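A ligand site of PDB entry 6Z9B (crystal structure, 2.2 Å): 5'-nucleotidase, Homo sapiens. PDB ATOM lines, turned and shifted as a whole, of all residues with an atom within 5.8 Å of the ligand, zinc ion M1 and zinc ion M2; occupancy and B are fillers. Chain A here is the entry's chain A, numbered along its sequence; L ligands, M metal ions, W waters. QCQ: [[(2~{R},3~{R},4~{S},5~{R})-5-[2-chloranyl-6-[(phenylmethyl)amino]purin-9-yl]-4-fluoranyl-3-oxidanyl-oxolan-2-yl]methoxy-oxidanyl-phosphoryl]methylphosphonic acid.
Water W5 lies within hydrogen-bond range of OD1 of Asn 220 (2.7 Å) and O1A of the ligand (2.7 Å). Water W3 bridges an oxygen (O1A) of the ligand (2.8 Å) and the guanidinium group of Arg 329 (3.3 Å). Water W10 lies within hydrogen-bond range of the backbone carbonyl oxygen (O) of Leu 159 (2.7 Å) and a nitrogen (N7) of the ligand (2.9 Å). Water W9 bridges the backbone carbonyl oxygen of Ser 219 and an oxygen (O2A) of the ligand. Water W4 bridges the backbone carbonyl oxygen of His 218 (3.1 Å) and an oxygen (O2A) of the ligand (3.5 Å).
An oxygen (O3') of the ligand sits at hydrogen-bond distance from the side-chain carboxylate (OD2) of Asp 481, at 2.7 Å. The guanidinium group of Arg 370 is in salt-bridge range of an oxygen (O1B) of the ligand, 3.2 Å away. NH1 of Arg 329 is in salt-bridge range of O2A of the ligand (3.1 Å). A nitrogen (N3) of the ligand is in hydrogen-bond range of the side-chain amide nitrogen of Asn 365 (3.4 Å). O3' of the ligand lies close to O of Gly 422 (3.1 Å). An oxygen (O1B) of the ligand is in hydrogen-bond range of a ring nitrogen (NE2) of His 93, at 2.7 Å. ND2 of Asn 220 lies within hydrogen-bond range of O1A of the ligand (3.1 Å).
Of the 34 residues printed, 5 come within 4 Å of zinc ion M2. The nearest printed residue that does not touch zinc ion M2 is His 93 (4.2 Å).
The backbone carbonyl oxygen (O) of Gly 367 lies close to an oxygen (O4') of the ligand (2.9 Å). Residues that only touch the ligand: Asp 96, Leu 159, Ser 160, Asn 161, Gly 368, Phe 392, Glu 423, Pro 473 and Phe 475. 22 residues have an atom within 4 Å of the ligand: Asp 11, His 13, Asp 60, Asn 92, His 93, Asp 96, Leu 159, Ser 160, Asn 161, His 218, Asn 220, Arg 329, Asn 365, Gly 367, Gly 368, Arg 370, Phe 392, Gly 422, Glu 423, Pro 473, Phe 475 and Asp 481.
The side-chain carboxylate (OD2) of Asp 96 sits at hydrogen-bond distance from a ring nitrogen (ND1) of His 93 (2.7 Å). The backbone carbonyl oxygen of Ser 420 sits at hydrogen-bond distance from the guanidinium group of Arg 329 (2.8 Å). The side-chain amide nitrogen of Gln 63 lies within hydrogen-bond range of the side-chain carboxylate of Asp 96 (2.8 Å). The backbone NH (N) of His 93 is in hydrogen-bond range of the side-chain carboxylate (OD1) of Asp 60 (2.9 Å). N of Asp 11 sits at hydrogen-bond distance from O of Gly 59 (2.9 Å). The side-chain carboxylate (OD1) of Asp 96 is in hydrogen-bond range of the side-chain hydroxyl (OG) of Ser 160 (2.9 Å). The backbone carbonyl oxygen (O) of Asn 92 sits at hydrogen-bond distance from the side-chain hydroxyl (OG) of Ser 160, 3.0 Å away. The backbone carbonyl oxygen of Phe 95 lies close to the side-chain hydroxyl of Ser 160 (3.2 Å).
Zinc ion M1 is bound by NE2 of His 13 (2.1 Å), OD2 of Asp 11 (2.1 Å), O3B of the ligand (2.1 Å), water W5 (2.1 Å) and OD2 of Asp 60 (2.3 Å).
Zinc ion M2 is bound by O2B of the ligand (1.9 Å), NE2 of His 195 (2.1 Å), OD2 of Asp 60 (2.1 Å), OD1 of Asn 92 (2.1 Å) and ND1 of His 218 (2.2 Å).
Three residues have an atom within 4 Å of zinc ion M1: Asp 11, His 13 and Asp 60. The nearest printed residue that does not touch zinc ion M1 is Arg 370 (4.1 Å).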
ATOM      1  N   ASP A  11      23.169  17.987  33.264  1.00  0.00           N
ATOM      2  CA  ASP A  11      23.279  18.679  31.986  1.00  0.00           C
ATOM      3  C   ASP A  11      24.642  19.351  31.784  1.00  0.00           C
ATOM      4  O   ASP A  11      24.726  20.487  31.328  1.00  0.00           O
ATOM      5  CB  ASP A  11      22.103  19.664  31.822  1.00  0.00           C
ATOM      6  CG  ASP A  11      20.776  18.958  32.009  1.00  0.00           C
ATOM      7  OD1 ASP A  11      20.352  18.798  33.169  1.00  0.00           O
ATOM      8  OD2 ASP A  11      20.203  18.497  31.015  1.00  0.00           O
ATOM      9  N   HIS A  13      26.957  18.361  29.679  1.00  0.00           N
ATOM     10  CA  HIS A  13      27.025  18.449  28.224  1.00  0.00           C
ATOM     11  C   HIS A  13      28.456  18.664  27.644  1.00  0.00           C
ATOM     12  O   HIS A  13      28.692  19.628  26.905  1.00  0.00           O
ATOM     13  CB  HIS A  13      26.030  19.516  27.673  1.00  0.00           C
ATOM     14  CG  HIS A  13      24.611  19.023  27.677  1.00  0.00           C
ATOM     15  ND1 HIS A  13      24.229  17.934  26.925  1.00  0.00           N
ATOM     16  CD2 HIS A  13      23.552  19.450  28.395  1.00  0.00           C
ATOM     17  CE1 HIS A  13      22.937  17.763  27.173  1.00  0.00           C
ATOM     18  NE2 HIS A  13      22.485  18.628  28.064  1.00  0.00           N
ATOM     19  N   GLY A  59      21.970  13.136  34.737  1.00  0.00           N
ATOM     20  CA  GLY A  59      21.819  12.974  33.295  1.00  0.00           C
ATOM     21  C   GLY A  59      22.376  14.049  32.397  1.00  0.00           C
ATOM     22  O   GLY A  59      22.787  15.123  32.855  1.00  0.00           O
ATOM     23  N   ASP A  60      22.386  13.754  31.095  1.00  0.00           N
ATOM     24  CA  ASP A  60      22.838  14.607  29.992  1.00  0.00           C
ATOM     25  C   ASP A  60      24.317  15.061  30.123  1.00  0.00           C
ATOM     26  O   ASP A  60      24.631  16.261  30.135  1.00  0.00           O
ATOM     27  CB  ASP A  60      21.887  15.782  29.763  1.00  0.00           C
ATOM     28  CG  ASP A  60      20.630  15.503  28.962  1.00  0.00           C
ATOM     29  OD1 ASP A  60      20.453  14.357  28.504  1.00  0.00           O
ATOM     30  OD2 ASP A  60      19.804  16.447  28.801  1.00  0.00           O
ATOM     31  N   GLN A  63      26.726  14.876  24.649  1.00  0.00           N
ATOM     32  CA  GLN A  63      26.435  15.915  23.642  1.00  0.00           C
ATOM     33  C   GLN A  63      26.718  17.367  24.045  1.00  0.00           C
ATOM     34  O   GLN A  63      26.173  17.841  25.029  1.00  0.00           O
ATOM     35  CB  GLN A  63      24.979  15.797  23.138  1.00  0.00           C
ATOM     36  CG  GLN A  63      24.780  16.240  21.695  1.00  0.00           C
ATOM     37  CD  GLN A  63      25.362  15.243  20.731  1.00  0.00           C
ATOM     38  OE1 GLN A  63      26.516  15.345  20.327  1.00  0.00           O
ATOM     39  NE2 GLN A  63      24.576  14.264  20.335  1.00  0.00           N
ATOM     40  N   GLY A  91      20.001  10.166  31.064  1.00  0.00           N
ATOM     41  CA  GLY A  91      19.315  11.306  30.466  1.00  0.00           C
ATOM     42  C   GLY A  91      18.981  11.021  29.007  1.00  0.00           C
ATOM     43  O   GLY A  91      19.464  10.026  28.461  1.00  0.00           O
ATOM     44  N   ASN A  92      18.159  11.859  28.374  1.00  0.00           N
ATOM     45  CA  ASN A  92      17.779  11.653  26.962  1.00  0.00           C
ATOM     46  C   ASN A  92      18.933  11.729  25.970  1.00  0.00           C
ATOM     47  O   ASN A  92      18.949  10.961  25.019  1.00  0.00           O
ATOM     48  CB  ASN A  92      16.643  12.607  26.517  1.00  0.00           C
ATOM     49  CG  ASN A  92      16.894  14.068  26.798  1.00  0.00           C
ATOM     50  OD1 ASN A  92      16.793  14.536  27.938  1.00  0.00           O
ATOM     51  ND2 ASN A  92      17.214  14.834  25.767  1.00  0.00           N
ATOM     52  N   HIS A  93      19.930  12.634  26.199  1.00  0.00           N
ATOM     53  CA  HIS A  93      21.067  12.790  25.287  1.00  0.00           C
ATOM     54  C   HIS A  93      22.051  11.589  25.313  1.00  0.00           C
ATOM     55  O   HIS A  93      22.797  11.415  24.352  1.00  0.00           O
ATOM     56  CB  HIS A  93      21.771  14.132  25.490  1.00  0.00           C
ATOM     57  CG  HIS A  93      20.963  15.269  24.946  1.00  0.00           C
ATOM     58  ND1 HIS A  93      20.790  15.436  23.593  1.00  0.00           N
ATOM     59  CD2 HIS A  93      20.263  16.230  25.588  1.00  0.00           C
ATOM     60  CE1 HIS A  93      20.013  16.485  23.446  1.00  0.00           C
ATOM     61  NE2 HIS A  93      19.702  17.019  24.615  1.00  0.00           N
ATOM     62  N   PHE A  95      21.179   8.701  24.687  1.00  0.00           N
ATOM     63  CA  PHE A  95      20.632   7.854  23.626  1.00  0.00           C
ATOM     64  C   PHE A  95      20.837   8.441  22.227  1.00  0.00           C
ATOM     65  O   PHE A  95      20.385   7.824  21.268  1.00  0.00           O
ATOM     66  CB  PHE A  95      19.123   7.582  23.888  1.00  0.00           C
ATOM     67  CG  PHE A  95      18.878   6.814  25.172  1.00  0.00           C
ATOM     68  CD1 PHE A  95      18.863   5.414  25.174  1.00  0.00           C
ATOM     69  CD2 PHE A  95      18.697   7.489  26.379  1.00  0.00           C
ATOM     70  CE1 PHE A  95      18.677   4.704  26.367  1.00  0.00           C
ATOM     71  CE2 PHE A  95      18.557   6.766  27.579  1.00  0.00           C
ATOM     72  CZ  PHE A  95      18.537   5.383  27.557  1.00  0.00           C
ATOM     73  N   ASP A  96      21.491   9.631  22.094  1.00  0.00           N
ATOM     74  CA  ASP A  96      21.682  10.346  20.807  1.00  0.00           C
ATOM     75  C   ASP A  96      22.437   9.546  19.742  1.00  0.00           C
ATOM     76  O   ASP A  96      22.299   9.823  18.542  1.00  0.00           O
ATOM     77  CB  ASP A  96      22.399  11.697  21.026  1.00  0.00           C
ATOM     78  CG  ASP A  96      21.585  12.844  21.592  1.00  0.00           C
ATOM     79  OD1 ASP A  96      20.380  12.640  21.901  1.00  0.00           O
ATOM     80  OD2 ASP A  96      22.144  13.952  21.722  1.00  0.00           O
ATOM     81  N   ASN A  97      23.286   8.611  20.185  1.00  0.00           N
ATOM     82  CA  ASN A  97      24.077   7.750  19.304  1.00  0.00           C
ATOM     83  C   ASN A  97      23.511   6.318  19.346  1.00  0.00           C
ATOM     84  O   ASN A  97      24.246   5.350  19.203  1.00  0.00           O
ATOM     85  CB  ASN A  97      25.563   7.797  19.743  1.00  0.00           C
ATOM     86  CG  ASN A  97      26.297   9.072  19.339  1.00  0.00           C
ATOM     87  OD1 ASN A  97      25.785   9.911  18.585  1.00  0.00           O
ATOM     88  ND2 ASN A  97      27.514   9.254  19.815  1.00  0.00           N
ATOM     89  N   PHE A 158      11.022  10.796  21.585  1.00  0.00           N
ATOM     90  CA  PHE A 158      10.824  11.981  20.734  1.00  0.00           C
ATOM     91  C   PHE A 158      12.010  12.938  20.822  1.00  0.00           C
ATOM     92  O   PHE A 158      12.214  13.744  19.910  1.00  0.00           O
ATOM     93  CB  PHE A 158       9.529  12.740  21.105  1.00  0.00           C
ATOM     94  CG  PHE A 158       8.304  11.866  21.200  1.00  0.00           C
ATOM     95  CD1 PHE A 158       7.656  11.410  20.052  1.00  0.00           C
ATOM     96  CD2 PHE A 158       7.822  11.446  22.439  1.00  0.00           C
ATOM     97  CE1 PHE A 158       6.546  10.573  20.141  1.00  0.00           C
ATOM     98  CE2 PHE A 158       6.714  10.599  22.520  1.00  0.00           C
ATOM     99  CZ  PHE A 158       6.082  10.169  21.375  1.00  0.00           C
ATOM    100  N   LEU A 159      12.775  12.869  21.930  1.00  0.00           N
ATOM    101  CA  LEU A 159      13.948  13.730  22.137  1.00  0.00           C
ATOM    102  C   LEU A 159      15.238  13.144  21.555  1.00  0.00           C
ATOM    103  O   LEU A 159      16.132  13.899  21.191  1.00  0.00           O
ATOM    104  CB  LEU A 159      14.173  14.051  23.638  1.00  0.00           C
ATOM    105  CG  LEU A 159      12.978  14.514  24.486  1.00  0.00           C
ATOM    106  CD1 LEU A 159      13.401  14.723  25.930  1.00  0.00           C
ATOM    107  CD2 LEU A 159      12.337  15.777  23.927  1.00  0.00           C
ATOM    108  N   SER A 160      15.343  11.818  21.478  1.00  0.00           N
ATOM    109  CA  SER A 160      16.571  11.133  21.094  1.00  0.00           C
ATOM    110  C   SER A 160      16.415   9.995  20.080  1.00  0.00           C
ATOM    111  O   SER A 160      15.493  10.003  19.261  1.00  0.00           O
ATOM    112  CB  SER A 160      17.257  10.641  22.356  1.00  0.00           C
ATOM    113  OG  SER A 160      18.629  10.386  22.115  1.00  0.00           O
ATOM    114  N   ASN A 161      17.350   9.014  20.103  1.00  0.00           N
ATOM    115  CA  ASN A 161      17.343   7.834  19.232  1.00  0.00           C
ATOM    116  C   ASN A 161      17.507   6.540  20.076  1.00  0.00           C
ATOM    117  O   ASN A 161      18.468   5.792  19.862  1.00  0.00           O
ATOM    118  CB  ASN A 161      18.417   7.973  18.137  1.00  0.00           C
ATOM    119  CG  ASN A 161      18.264   7.047  16.961  1.00  0.00           C
ATOM    120  OD1 ASN A 161      17.170   6.574  16.636  1.00  0.00           O
ATOM    121  ND2 ASN A 161      19.373   6.786  16.272  1.00  0.00           N
ATOM    122  N   HIS A 195      16.249  12.241  35.283  1.00  0.00           N
ATOM    123  CA  HIS A 195      16.255  13.178  34.186  1.00  0.00           C
ATOM    124  C   HIS A 195      14.900  13.476  33.458  1.00  0.00           C
ATOM    125  O   HIS A 195      14.763  13.162  32.276  1.00  0.00           O
ATOM    126  CB  HIS A 195      17.282  12.687  33.175  1.00  0.00           C
ATOM    127  CG  HIS A 195      17.756  13.779  32.289  1.00  0.00           C
ATOM    128  ND1 HIS A 195      18.778  14.609  32.670  1.00  0.00           N
ATOM    129  CD2 HIS A 195      17.270  14.186  31.097  1.00  0.00           C
ATOM    130  CE1 HIS A 195      18.916  15.477  31.688  1.00  0.00           C
ATOM    131  NE2 HIS A 195      18.012  15.268  30.733  1.00  0.00           N
ATOM    132  N   HIS A 218      17.578  18.018  33.243  1.00  0.00           N
ATOM    133  CA  HIS A 218      16.786  18.267  31.994  1.00  0.00           C
ATOM    134  C   HIS A 218      16.215  19.694  31.824  1.00  0.00           C
ATOM    135  O   HIS A 218      16.197  20.182  30.697  1.00  0.00           O
ATOM    136  CB  HIS A 218      15.673  17.208  31.838  1.00  0.00           C
ATOM    137  CG  HIS A 218      14.976  17.223  30.503  1.00  0.00           C
ATOM    138  ND1 HIS A 218      15.678  17.142  29.308  1.00  0.00           N
ATOM    139  CD2 HIS A 218      13.652  17.333  30.227  1.00  0.00           C
ATOM    140  CE1 HIS A 218      14.768  17.186  28.353  1.00  0.00           C
ATOM    141  NE2 HIS A 218      13.538  17.299  28.852  1.00  0.00           N
ATOM    142  N   SER A 219      15.731  20.353  32.861  1.00  0.00           N
ATOM    143  CA  SER A 219      15.165  21.721  32.712  1.00  0.00           C
ATOM    144  C   SER A 219      16.198  22.825  33.031  1.00  0.00           C
ATOM    145  O   SER A 219      15.859  24.026  32.965  1.00  0.00           O
ATOM    146  CB  SER A 219      13.918  21.895  33.582  1.00  0.00           C
ATOM    147  OG  SER A 219      14.088  21.379  34.896  1.00  0.00           O
ATOM    148  N   ASN A 220      17.458  22.417  33.336  1.00  0.00           N
ATOM    149  CA  ASN A 220      18.596  23.307  33.666  1.00  0.00           C
ATOM    150  C   ASN A 220      18.235  24.296  34.784  1.00  0.00           C
ATOM    151  O   ASN A 220      18.690  25.444  34.762  1.00  0.00           O
ATOM    152  CB  ASN A 220      19.069  24.062  32.410  1.00  0.00           C
ATOM    153  CG  ASN A 220      19.396  23.188  31.230  1.00  0.00           C
ATOM    154  OD1 ASN A 220      20.108  22.207  31.372  1.00  0.00           O
ATOM    155  ND2 ASN A 220      18.874  23.534  30.052  1.00  0.00           N
ATOM    156  N   ARG A 329      15.856  31.753  23.184  1.00  0.00           N
ATOM    157  CA  ARG A 329      14.564  31.158  23.548  1.00  0.00           C
ATOM    158  C   ARG A 329      13.529  32.253  23.945  1.00  0.00           C
ATOM    159  O   ARG A 329      12.373  31.924  24.235  1.00  0.00           O
ATOM    160  CB  ARG A 329      14.742  30.180  24.735  1.00  0.00           C
ATOM    161  CG  ARG A 329      15.635  28.984  24.450  1.00  0.00           C
ATOM    162  CD  ARG A 329      15.553  27.965  25.578  1.00  0.00           C
ATOM    163  NE  ARG A 329      16.630  26.990  25.461  1.00  0.00           N
ATOM    164  CZ  ARG A 329      16.604  25.755  25.938  1.00  0.00           C
ATOM    165  NH1 ARG A 329      15.548  25.318  26.613  1.00  0.00           N
ATOM    166  NH2 ARG A 329      17.644  24.943  25.753  1.00  0.00           N
ATOM    167  N   ASN A 365      14.337  26.331  15.718  1.00  0.00           N
ATOM    168  CA  ASN A 365      14.044  26.276  17.158  1.00  0.00           C
ATOM    169  C   ASN A 365      15.246  26.832  17.934  1.00  0.00           C
ATOM    170  O   ASN A 365      16.377  26.365  17.747  1.00  0.00           O
ATOM    171  CB  ASN A 365      13.687  24.837  17.624  1.00  0.00           C
ATOM    172  CG  ASN A 365      14.723  23.779  17.312  1.00  0.00           C
ATOM    173  OD1 ASN A 365      15.176  23.614  16.173  1.00  0.00           O
ATOM    174  ND2 ASN A 365      15.098  23.014  18.331  1.00  0.00           N
ATOM    175  N   GLY A 366      14.985  27.851  18.752  1.00  0.00           N
ATOM    176  CA  GLY A 366      15.977  28.539  19.589  1.00  0.00           C
ATOM    177  C   GLY A 366      16.780  27.637  20.521  1.00  0.00           C
ATOM    178  O   GLY A 366      17.975  27.875  20.723  1.00  0.00           O
ATOM    179  N   GLY A 367      16.144  26.574  21.028  1.00  0.00           N
ATOM    180  CA  GLY A 367      16.752  25.569  21.898  1.00  0.00           C
ATOM    181  C   GLY A 367      17.728  24.633  21.193  1.00  0.00           C
ATOM    182  O   GLY A 367      18.498  23.933  21.853  1.00  0.00           O
ATOM    183  N   GLY A 368      17.714  24.640  19.853  1.00  0.00           N
ATOM    184  CA  GLY A 368      18.664  23.881  19.039  1.00  0.00           C
ATOM    185  C   GLY A 368      20.033  24.562  18.963  1.00  0.00           C
ATOM    186  O   GLY A 368      21.005  23.920  18.564  1.00  0.00           O
ATOM    187  N   ARG A 370      23.075  25.691  20.838  1.00  0.00           N
ATOM    188  CA  ARG A 370      23.552  25.195  22.129  1.00  0.00           C
ATOM    189  C   ARG A 370      24.742  25.930  22.772  1.00  0.00           C
ATOM    190  O   ARG A 370      25.170  25.550  23.870  1.00  0.00           O
ATOM    191  CB  ARG A 370      23.843  23.679  22.030  1.00  0.00           C
ATOM    192  CG  ARG A 370      22.675  22.849  21.454  1.00  0.00           C
ATOM    193  CD  ARG A 370      21.492  22.671  22.394  1.00  0.00           C
ATOM    194  NE  ARG A 370      21.835  21.860  23.569  1.00  0.00           N
ATOM    195  CZ  ARG A 370      20.958  21.173  24.292  1.00  0.00           C
ATOM    196  NH1 ARG A 370      21.367  20.451  25.334  1.00  0.00           N
ATOM    197  NH2 ARG A 370      19.667  21.202  23.993  1.00  0.00           N
ATOM    198  N   PHE A 392      24.581  18.354  17.281  1.00  0.00           N
ATOM    199  CA  PHE A 392      23.737  17.187  17.010  1.00  0.00           C
ATOM    200  C   PHE A 392      23.906  16.466  15.678  1.00  0.00           C
ATOM    201  O   PHE A 392      23.367  15.362  15.535  1.00  0.00           O
ATOM    202  CB  PHE A 392      22.265  17.561  17.176  1.00  0.00           C
ATOM    203  CG  PHE A 392      21.933  18.263  18.474  1.00  0.00           C
ATOM    204  CD1 PHE A 392      22.068  17.607  19.688  1.00  0.00           C
ATOM    205  CD2 PHE A 392      21.460  19.578  18.467  1.00  0.00           C
ATOM    206  CE1 PHE A 392      21.727  18.247  20.884  1.00  0.00           C
ATOM    207  CE2 PHE A 392      21.082  20.192  19.664  1.00  0.00           C
ATOM    208  CZ  PHE A 392      21.227  19.520  20.866  1.00  0.00           C
ATOM    209  N   SER A 420      11.404  29.288  29.260  1.00  0.00           N
ATOM    210  CA  SER A 420      12.737  28.972  28.706  1.00  0.00           C
ATOM    211  C   SER A 420      12.657  27.694  27.865  1.00  0.00           C
ATOM    212  O   SER A 420      13.557  26.840  27.858  1.00  0.00           O
ATOM    213  CB  SER A 420      13.819  28.908  29.779  1.00  0.00           C
ATOM    214  OG  SER A 420      15.085  28.855  29.143  1.00  0.00           O
ATOM    215  N   THR A 421      11.531  27.582  27.180  1.00  0.00           N
ATOM    216  CA  THR A 421      11.213  26.498  26.276  1.00  0.00           C
ATOM    217  C   THR A 421      11.908  26.834  24.936  1.00  0.00           C
ATOM    218  O   THR A 421      11.824  27.972  24.412  1.00  0.00           O
ATOM    219  CB  THR A 421       9.680  26.287  26.207  1.00  0.00           C
ATOM    220  OG1 THR A 421       9.009  27.536  25.970  1.00  0.00           O
ATOM    221  CG2 THR A 421       9.122  25.590  27.455  1.00  0.00           C
ATOM    222  N   GLY A 422      12.631  25.839  24.425  1.00  0.00           N
ATOM    223  CA  GLY A 422      13.415  25.942  23.206  1.00  0.00           C
ATOM    224  C   GLY A 422      12.671  26.006  21.899  1.00  0.00           C
ATOM    225  O   GLY A 422      13.328  26.101  20.852  1.00  0.00           O
ATOM    226  N   GLU A 423      11.327  25.962  21.911  1.00  0.00           N
ATOM    227  CA  GLU A 423      10.511  25.994  20.691  1.00  0.00           C
ATOM    228  C   GLU A 423      10.419  27.395  20.077  1.00  0.00           C
ATOM    229  O   GLU A 423       9.980  27.500  18.942  1.00  0.00           O
ATOM    230  CB  GLU A 423       9.125  25.363  20.876  1.00  0.00           C
ATOM    231  CG  GLU A 423       8.132  26.213  21.661  1.00  0.00           C
ATOM    232  CD  GLU A 423       7.952  25.781  23.098  1.00  0.00           C
ATOM    233  OE1 GLU A 423       6.888  26.097  23.670  1.00  0.00           O
ATOM    234  OE2 GLU A 423       8.864  25.122  23.654  1.00  0.00           O
ATOM    235  N   PRO A 473      15.489  22.779  10.571  1.00  0.00           N
ATOM    236  CA  PRO A 473      16.188  21.538  10.978  1.00  0.00           C
ATOM    237  C   PRO A 473      15.318  20.295  10.759  1.00  0.00           C
ATOM    238  O   PRO A 473      14.096  20.357  10.908  1.00  0.00           O
ATOM    239  CB  PRO A 473      16.484  21.739  12.472  1.00  0.00           C
ATOM    240  CG  PRO A 473      16.245  23.186  12.748  1.00  0.00           C
ATOM    241  CD  PRO A 473      15.258  23.673  11.725  1.00  0.00           C
ATOM    242  N   ASN A 474      15.952  19.154  10.443  1.00  0.00           N
ATOM    243  CA  ASN A 474      15.312  17.850  10.279  1.00  0.00           C
ATOM    244  C   ASN A 474      14.456  17.519  11.539  1.00  0.00           C
ATOM    245  O   ASN A 474      13.421  16.856  11.429  1.00  0.00           O
ATOM    246  CB  ASN A 474      16.360  16.742  10.042  1.00  0.00           C
ATOM    247  CG  ASN A 474      17.332  16.490  11.188  1.00  0.00           C
ATOM    248  OD1 ASN A 474      17.753  17.399  11.934  1.00  0.00           O
ATOM    249  ND2 ASN A 474      17.735  15.233  11.340  1.00  0.00           N
ATOM    250  N   PHE A 475      14.893  18.047  12.708  1.00  0.00           N
ATOM    251  CA  PHE A 475      14.261  17.914  14.016  1.00  0.00           C
ATOM    252  C   PHE A 475      12.849  18.500  14.036  1.00  0.00           C
ATOM    253  O   PHE A 475      11.955  17.920  14.638  1.00  0.00           O
ATOM    254  CB  PHE A 475      15.145  18.611  15.070  1.00  0.00           C
ATOM    255  CG  PHE A 475      14.672  18.486  16.491  1.00  0.00           C
ATOM    256  CD1 PHE A 475      14.880  17.318  17.219  1.00  0.00           C
ATOM    257  CD2 PHE A 475      14.047  19.569  17.131  1.00  0.00           C
ATOM    258  CE1 PHE A 475      14.444  17.218  18.542  1.00  0.00           C
ATOM    259  CE2 PHE A 475      13.620  19.458  18.458  1.00  0.00           C
ATOM    260  CZ  PHE A 475      13.830  18.279  19.154  1.00  0.00           C
ATOM    261  N   ASP A 481      10.014  19.261  19.271  1.00  0.00           N
ATOM    262  CA  ASP A 481       9.703  20.470  20.066  1.00  0.00           C
ATOM    263  C   ASP A 481       8.204  20.823  20.052  1.00  0.00           C
ATOM    264  O   ASP A 481       7.842  21.977  20.285  1.00  0.00           O
ATOM    265  CB  ASP A 481      10.565  21.690  19.628  1.00  0.00           C
ATOM    266  CG  ASP A 481      11.612  22.108  20.628  1.00  0.00           C
ATOM    267  OD1 ASP A 481      11.578  21.621  21.775  1.00  0.00           O
ATOM    268  OD2 ASP A 481      12.472  22.950  20.254  1.00  0.00           O
HETATM  269  O3' QCQ L   1      14.389  23.397  22.057  1.00  0.00           O
HETATM  270  C3' QCQ L   1      14.696  22.167  22.704  1.00  0.00           C
HETATM  271  C2' QCQ L   1      14.980  21.044  21.716  1.00  0.00           C
HETATM  272  F04 QCQ L   1      14.765  19.817  22.349  1.00  0.00           F
HETATM  273  C4' QCQ L   1      15.993  22.236  23.528  1.00  0.00           C
HETATM  274  C5' QCQ L   1      15.898  21.609  24.894  1.00  0.00           C
HETATM  275  O5' QCQ L   1      17.174  21.700  25.530  1.00  0.00           O
HETATM  276  PA  QCQ L   1      17.276  21.663  27.102  1.00  0.00           P
HETATM  277  C3A QCQ L   1      16.936  19.950  27.565  1.00  0.00           C
HETATM  278  PB  QCQ L   1      18.009  18.769  26.765  1.00  0.00           P
HETATM  279  O1B QCQ L   1      17.832  18.885  25.282  1.00  0.00           O
HETATM  280  O2B QCQ L   1      17.720  17.352  27.296  1.00  0.00           O
HETATM  281  O3B QCQ L   1      19.435  19.152  27.232  1.00  0.00           O
HETATM  282  O1A QCQ L   1      18.778  21.959  27.391  1.00  0.00           O
HETATM  283  O2A QCQ L   1      16.423  22.668  27.859  1.00  0.00           O
HETATM  284  O4' QCQ L   1      17.005  21.557  22.757  1.00  0.00           O
HETATM  285  C1' QCQ L   1      16.472  21.195  21.496  1.00  0.00           C
HETATM  286  N9  QCQ L   1      17.136  19.981  21.018  1.00  0.00           N
HETATM  287  C8  QCQ L   1      17.613  18.938  21.763  1.00  0.00           C
HETATM  288  N7  QCQ L   1      18.158  17.984  21.052  1.00  0.00           N
HETATM  289  C5  QCQ L   1      18.026  18.427  19.743  1.00  0.00           C
HETATM  290  C4  QCQ L   1      17.417  19.669  19.711  1.00  0.00           C
HETATM  291  N3  QCQ L   1      17.222  20.438  18.630  1.00  0.00           N
HETATM  292  C2  QCQ L   1      17.710  19.856  17.546  1.00  0.00           C
HETATM  293 CL1  QCQ L   1      17.674  20.838  16.097  1.00  0.00          CL
HETATM  294  N1  QCQ L   1      18.282  18.673  17.394  1.00  0.00           N
HETATM  295  C6  QCQ L   1      18.454  17.912  18.496  1.00  0.00           C
HETATM  296  N6  QCQ L   1      19.080  16.718  18.364  1.00  0.00           N
HETATM  297  C29 QCQ L   1      18.947  15.626  19.317  1.00  0.00           C
HETATM  298  C30 QCQ L   1      18.818  14.257  18.691  1.00  0.00           C
HETATM  299  C31 QCQ L   1      17.562  13.732  18.392  1.00  0.00           C
HETATM  300  C32 QCQ L   1      17.440  12.466  17.846  1.00  0.00           C
HETATM  301  C33 QCQ L   1      18.573  11.691  17.611  1.00  0.00           C
HETATM  302  C34 QCQ L   1      19.822  12.209  17.906  1.00  0.00           C
HETATM  303  C35 QCQ L   1      19.944  13.480  18.444  1.00  0.00           C
HETATM  304 ZN    ZN M   1      20.629  18.643  28.936  1.00  0.00          ZN
HETATM  305 ZN    ZN M   2      17.676  16.248  28.882  1.00  0.00          ZN
HETATM  306  O   HOH W   1      19.341  15.550  15.458  1.00  0.00           O
HETATM  307  O   HOH W   2      11.605  18.971  22.973  1.00  0.00           O
HETATM  308  O   HOH W   3      20.643  24.010  26.902  1.00  0.00           O
HETATM  309  O   HOH W   4      13.640  21.071  29.244  1.00  0.00           O
HETATM  310  O   HOH W   5      20.505  20.777  29.131  1.00  0.00           O
HETATM  311  O   HOH W   6      15.431  17.663  24.662  1.00  0.00           O
HETATM  312  O   HOH W   7      19.444  18.233  15.002  1.00  0.00           O
HETATM  313  O   HOH W   8      13.224  18.949  25.177  1.00  0.00           O
HETATM  314  O   HOH W   9      15.321  24.562  30.060  1.00  0.00           O
HETATM  315  O   HOH W  10      15.858  16.477  22.009  1.00  0.00           O
